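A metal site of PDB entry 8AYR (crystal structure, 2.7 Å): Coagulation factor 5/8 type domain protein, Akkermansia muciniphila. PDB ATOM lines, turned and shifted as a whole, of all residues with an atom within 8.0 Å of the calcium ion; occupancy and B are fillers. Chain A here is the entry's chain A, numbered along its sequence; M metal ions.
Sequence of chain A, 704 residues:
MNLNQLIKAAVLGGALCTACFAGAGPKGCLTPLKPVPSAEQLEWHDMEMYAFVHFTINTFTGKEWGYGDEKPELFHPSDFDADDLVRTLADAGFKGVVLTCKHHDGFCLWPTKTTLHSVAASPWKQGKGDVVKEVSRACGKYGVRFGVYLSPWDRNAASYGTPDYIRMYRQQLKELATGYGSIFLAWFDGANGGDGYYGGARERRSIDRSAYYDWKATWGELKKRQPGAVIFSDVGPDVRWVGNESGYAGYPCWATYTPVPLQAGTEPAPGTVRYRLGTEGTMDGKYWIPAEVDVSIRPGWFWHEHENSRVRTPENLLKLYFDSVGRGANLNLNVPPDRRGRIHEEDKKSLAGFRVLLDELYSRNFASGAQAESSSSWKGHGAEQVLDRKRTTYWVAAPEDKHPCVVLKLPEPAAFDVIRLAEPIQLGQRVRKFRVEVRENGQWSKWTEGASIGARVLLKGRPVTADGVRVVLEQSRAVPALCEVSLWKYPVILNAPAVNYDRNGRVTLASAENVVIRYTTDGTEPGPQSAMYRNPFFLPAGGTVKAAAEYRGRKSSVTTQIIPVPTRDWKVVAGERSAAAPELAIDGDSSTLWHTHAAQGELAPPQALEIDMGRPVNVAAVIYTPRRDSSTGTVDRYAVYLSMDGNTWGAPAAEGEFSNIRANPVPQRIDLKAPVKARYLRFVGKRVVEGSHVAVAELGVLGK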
ATOM      1  N   ALA A 581     -26.461   1.459   6.818  1.00  0.00           N
ATOM      2  CA  ALA A 581     -25.098   1.482   7.347  1.00  0.00           C
ATOM      3  C   ALA A 581     -24.267   0.387   6.683  1.00  0.00           C
ATOM      4  O   ALA A 581     -24.621  -0.791   6.797  1.00  0.00           O
ATOM      5  CB  ALA A 581     -25.102   1.303   8.857  1.00  0.00           C
ATOM      6  N   PRO A 582     -23.189   0.731   5.980  1.00  0.00           N
ATOM      7  CA  PRO A 582     -22.386  -0.303   5.310  1.00  0.00           C
ATOM      8  C   PRO A 582     -21.853  -1.371   6.242  1.00  0.00           C
ATOM      9  O   PRO A 582     -21.578  -2.483   5.791  1.00  0.00           O
ATOM     10  CB  PRO A 582     -21.239   0.501   4.662  1.00  0.00           C
ATOM     11  CG  PRO A 582     -21.804   1.880   4.507  1.00  0.00           C
ATOM     12  CD  PRO A 582     -22.690   2.089   5.702  1.00  0.00           C
ATOM     13  N   GLU A 583     -21.703  -1.061   7.535  1.00  0.00           N
ATOM     14  CA  GLU A 583     -21.234  -2.069   8.482  1.00  0.00           C
ATOM     15  C   GLU A 583     -22.212  -3.234   8.611  1.00  0.00           C
ATOM     16  O   GLU A 583     -21.838  -4.267   9.199  1.00  0.00           O
ATOM     17  CB  GLU A 583     -21.003  -1.425   9.859  1.00  0.00           C
ATOM     18  CG  GLU A 583     -19.836  -0.438   9.874  1.00  0.00           C
ATOM     19  CD  GLU A 583     -20.255   0.955   9.433  1.00  0.00           C
ATOM     20  OE1 GLU A 583     -21.465   1.213   9.320  1.00  0.00           O
ATOM     21  OE2 GLU A 583     -19.364   1.788   9.187  1.00  0.00           O
ATOM     22  N   LEU A 584     -23.428  -3.114   8.078  1.00  0.00           N
ATOM     23  CA  LEU A 584     -24.359  -4.241   8.062  1.00  0.00           C
ATOM     24  C   LEU A 584     -23.960  -5.317   7.057  1.00  0.00           C
ATOM     25  O   LEU A 584     -24.560  -6.389   7.057  1.00  0.00           O
ATOM     26  CB  LEU A 584     -25.766  -3.749   7.753  1.00  0.00           C
ATOM     27  CG  LEU A 584     -26.393  -2.806   8.774  1.00  0.00           C
ATOM     28  CD1 LEU A 584     -27.779  -2.383   8.300  1.00  0.00           C
ATOM     29  CD2 LEU A 584     -26.443  -3.433  10.147  1.00  0.00           C
ATOM     30  N   ALA A 585     -22.975  -5.057   6.200  1.00  0.00           N
ATOM     31  CA  ALA A 585     -22.484  -6.055   5.258  1.00  0.00           C
ATOM     32  C   ALA A 585     -21.268  -6.813   5.777  1.00  0.00           C
ATOM     33  O   ALA A 585     -20.779  -7.718   5.089  1.00  0.00           O
ATOM     34  CB  ALA A 585     -22.151  -5.402   3.920  1.00  0.00           C
ATOM     35  N   ILE A 586     -20.759  -6.461   6.960  1.00  0.00           N
ATOM     36  CA  ILE A 586     -19.620  -7.158   7.560  1.00  0.00           C
ATOM     37  C   ILE A 586     -19.866  -7.398   9.042  1.00  0.00           C
ATOM     38  O   ILE A 586     -18.921  -7.487   9.834  1.00  0.00           O
ATOM     39  CB  ILE A 586     -18.302  -6.380   7.348  1.00  0.00           C
ATOM     40  CG1 ILE A 586     -18.408  -4.971   7.935  1.00  0.00           C
ATOM     41  CG2 ILE A 586     -17.902  -6.364   5.876  1.00  0.00           C
ATOM     42  CD1 ILE A 586     -17.087  -4.249   7.974  1.00  0.00           C
ATOM     43  N   ASP A 587     -21.139  -7.481   9.440  1.00  0.00           N
ATOM     44  CA  ASP A 587     -21.488  -7.744  10.831  1.00  0.00           C
ATOM     45  C   ASP A 587     -21.691  -9.236  11.123  1.00  0.00           C
ATOM     46  O   ASP A 587     -22.091  -9.580  12.240  1.00  0.00           O
ATOM     47  CB  ASP A 587     -22.753  -6.961  11.208  1.00  0.00           C
ATOM     48  CG  ASP A 587     -23.957  -7.336  10.363  1.00  0.00           C
ATOM     49  OD1 ASP A 587     -23.816  -8.137   9.424  1.00  0.00           O
ATOM     50  OD2 ASP A 587     -25.051  -6.814  10.668  1.00  0.00           O
ATOM     51  N   GLY A 588     -21.406 -10.111  10.165  1.00  0.00           N
ATOM     52  CA  GLY A 588     -21.553 -11.529  10.373  1.00  0.00           C
ATOM     53  C   GLY A 588     -22.976 -12.037  10.465  1.00  0.00           C
ATOM     54  O   GLY A 588     -23.183 -13.239  10.684  1.00  0.00           O
ATOM     55  N   ASP A 589     -23.981 -11.173  10.282  1.00  0.00           N
ATOM     56  CA  ASP A 589     -25.386 -11.562  10.364  1.00  0.00           C
ATOM     57  C   ASP A 589     -25.968 -11.477   8.953  1.00  0.00           C
ATOM     58  O   ASP A 589     -26.052 -10.392   8.379  1.00  0.00           O
ATOM     59  CB  ASP A 589     -26.164 -10.674  11.320  1.00  0.00           C
ATOM     60  CG  ASP A 589     -27.564 -11.205  11.611  1.00  0.00           C
ATOM     61  OD1 ASP A 589     -27.904 -12.279  11.078  1.00  0.00           O
ATOM     62  OD2 ASP A 589     -28.316 -10.549  12.359  1.00  0.00           O
ATOM     63  N   SER A 590     -26.366 -12.630   8.413  1.00  0.00           N
ATOM     64  CA  SER A 590     -26.940 -12.678   7.072  1.00  0.00           C
ATOM     65  C   SER A 590     -28.353 -12.089   7.031  1.00  0.00           C
ATOM     66  O   SER A 590     -28.840 -11.784   5.939  1.00  0.00           O
ATOM     67  CB  SER A 590     -26.935 -14.118   6.566  1.00  0.00           C
ATOM     68  OG  SER A 590     -27.744 -14.946   7.383  1.00  0.00           O
ATOM     69  N   SER A 591     -29.003 -11.928   8.178  1.00  0.00           N
ATOM     70  CA  SER A 591     -30.327 -11.328   8.268  1.00  0.00           C
ATOM     71  C   SER A 591     -30.280  -9.810   8.369  1.00  0.00           C
ATOM     72  O   SER A 591     -31.328  -9.175   8.519  1.00  0.00           O
ATOM     73  CB  SER A 591     -31.098 -11.894   9.465  1.00  0.00           C
ATOM     74  OG  SER A 591     -30.513 -11.474  10.694  1.00  0.00           O
ATOM     75  N   THR A 592     -29.096  -9.201   8.305  1.00  0.00           N
ATOM     76  CA  THR A 592     -28.930  -7.761   8.297  1.00  0.00           C
ATOM     77  C   THR A 592     -28.484  -7.329   6.902  1.00  0.00           C
ATOM     78  O   THR A 592     -27.665  -8.000   6.272  1.00  0.00           O
ATOM     79  CB  THR A 592     -27.910  -7.286   9.326  1.00  0.00           C
ATOM     80  OG1 THR A 592     -26.631  -7.854   9.028  1.00  0.00           O
ATOM     81  CG2 THR A 592     -28.337  -7.712  10.724  1.00  0.00           C
ATOM     82  N   LEU A 593     -29.041  -6.219   6.421  1.00  0.00           N
ATOM     83  CA  LEU A 593     -28.999  -5.883   5.010  1.00  0.00           C
ATOM     84  C   LEU A 593     -28.397  -4.503   4.824  1.00  0.00           C
ATOM     85  O   LEU A 593     -28.906  -3.526   5.389  1.00  0.00           O
ATOM     86  CB  LEU A 593     -30.396  -5.916   4.397  1.00  0.00           C
ATOM     87  CG  LEU A 593     -31.108  -7.239   4.108  1.00  0.00           C
ATOM     88  CD1 LEU A 593     -31.588  -7.903   5.391  1.00  0.00           C
ATOM     89  CD2 LEU A 593     -32.278  -7.012   3.151  1.00  0.00           C
ATOM     90  N   TRP A 594     -27.329  -4.418   4.042  1.00  0.00           N
ATOM     91  CA  TRP A 594     -26.877  -3.151   3.486  1.00  0.00           C
ATOM     92  C   TRP A 594     -27.523  -2.960   2.123  1.00  0.00           C
ATOM     93  O   TRP A 594     -27.547  -3.884   1.308  1.00  0.00           O
ATOM     94  CB  TRP A 594     -25.362  -3.110   3.343  1.00  0.00           C
ATOM     95  CG  TRP A 594     -24.903  -1.846   2.698  1.00  0.00           C
ATOM     96  CD1 TRP A 594     -24.908  -0.600   3.244  1.00  0.00           C
ATOM     97  CD2 TRP A 594     -24.453  -1.691   1.349  1.00  0.00           C
ATOM     98  NE1 TRP A 594     -24.441   0.320   2.336  1.00  0.00           N
ATOM     99  CE2 TRP A 594     -24.155  -0.324   1.156  1.00  0.00           C
ATOM    100  CE3 TRP A 594     -24.252  -2.574   0.284  1.00  0.00           C
ATOM    101  CZ2 TRP A 594     -23.671   0.173  -0.040  1.00  0.00           C
ATOM    102  CZ3 TRP A 594     -23.781  -2.072  -0.910  1.00  0.00           C
ATOM    103  CH2 TRP A 594     -23.497  -0.712  -1.073  1.00  0.00           C
ATOM    104  N   THR A 625     -22.691 -12.890   0.348  1.00  0.00           N
ATOM    105  CA  THR A 625     -23.955 -13.466   0.779  1.00  0.00           C
ATOM    106  C   THR A 625     -25.088 -12.520   0.408  1.00  0.00           C
ATOM    107  O   THR A 625     -25.139 -11.400   0.959  1.00  0.00           O
ATOM    108  CB  THR A 625     -23.951 -13.732   2.281  1.00  0.00           C
ATOM    109  OG1 THR A 625     -22.865 -14.609   2.616  1.00  0.00           O
ATOM    110  CG2 THR A 625     -25.267 -14.375   2.711  1.00  0.00           C
ATOM    111  N   VAL A 696     -26.219  -5.860  -0.243  1.00  0.00           N
ATOM    112  CA  VAL A 696     -25.311  -6.897   0.231  1.00  0.00           C
ATOM    113  C   VAL A 696     -25.751  -7.317   1.632  1.00  0.00           C
ATOM    114  O   VAL A 696     -25.855  -6.470   2.528  1.00  0.00           O
ATOM    115  CB  VAL A 696     -23.848  -6.409   0.242  1.00  0.00           C
ATOM    116  CG1 VAL A 696     -22.929  -7.509   0.764  1.00  0.00           C
ATOM    117  CG2 VAL A 696     -23.422  -5.954  -1.142  1.00  0.00           C
ATOM    118  N   ALA A 697     -26.014  -8.614   1.804  1.00  0.00           N
ATOM    119  CA  ALA A 697     -26.327  -9.126   3.132  1.00  0.00           C
ATOM    120  C   ALA A 697     -25.062  -9.370   3.952  1.00  0.00           C
ATOM    121  O   ALA A 697     -24.955  -8.899   5.087  1.00  0.00           O
ATOM    122  CB  ALA A 697     -27.164 -10.402   3.038  1.00  0.00           C
ATOM    123  N   GLU A 698     -24.090 -10.093   3.392  1.00  0.00           N
ATOM    124  CA  GLU A 698     -22.803 -10.274   4.042  1.00  0.00           C
ATOM    125  C   GLU A 698     -21.676 -10.269   3.025  1.00  0.00           C
ATOM    126  O   GLU A 698     -21.868 -10.577   1.842  1.00  0.00           O
ATOM    127  CB  GLU A 698     -22.744 -11.567   4.871  1.00  0.00           C
ATOM    128  CG  GLU A 698     -23.427 -11.485   6.213  1.00  0.00           C
ATOM    129  CD  GLU A 698     -22.661 -10.603   7.181  1.00  0.00           C
ATOM    130  OE1 GLU A 698     -21.414 -10.561   7.106  1.00  0.00           O
ATOM    131  OE2 GLU A 698     -23.315  -9.936   8.015  1.00  0.00           O
ATOM    132  N   LEU A 699     -20.475  -9.975   3.510  1.00  0.00           N
ATOM    133  CA  LEU A 699     -19.278  -9.938   2.688  1.00  0.00           C
ATOM    134  C   LEU A 699     -18.127 -10.493   3.500  1.00  0.00           C
ATOM    135  O   LEU A 699     -17.767  -9.923   4.537  1.00  0.00           O
ATOM    136  CB  LEU A 699     -18.977  -8.511   2.214  1.00  0.00           C
ATOM    137  CG  LEU A 699     -17.819  -8.326   1.239  1.00  0.00           C
ATOM    138  CD1 LEU A 699     -18.125  -8.999  -0.088  1.00  0.00           C
ATOM    139  CD2 LEU A 699     -17.513  -6.849   1.044  1.00  0.00           C
HETATM  140 CA    CA M   1     -25.068  -8.437   7.351  1.00  0.00          CA
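The calcium ion is bound by the backbone carbonyl oxygen (O) of Leu 584 (2.1 Å), the backbone carbonyl oxygen (O) of Ala 697 (2.3 Å), the side-chain hydroxyl (OG1) of Thr 592 (2.4 Å), the side-chain carboxylate (OE2) of Glu 698 (2.4 Å), the backbone carbonyl oxygen (O) of Asp 589 (2.4 Å), the side-chain carboxylate (OD1) of Asp 587 (2.4 Å) and the backbone carbonyl oxygen (O) of Thr 592 (2.8 Å).
OD1 of Asp 589 lies within hydrogen-bond range of OG of Ser 591 (2.8 Å). N of Thr 625 sits at hydrogen-bond distance from O of Glu 698, at 2.9 Å. The backbone NH (N) of Gly 588 is in hydrogen-bond range of the side-chain carboxylate (OE1) of Glu 698 (3.1 Å). The backbone carbonyl oxygen (O) of Thr 625 lies within hydrogen-bond range of the backbone NH (N) of Ala 697 (3.0 Å).
Six residues have an atom within 4 Å of the calcium ion: Leu 584, Asp 587, Asp 589, Thr 592, Ala 697 and Glu 698.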
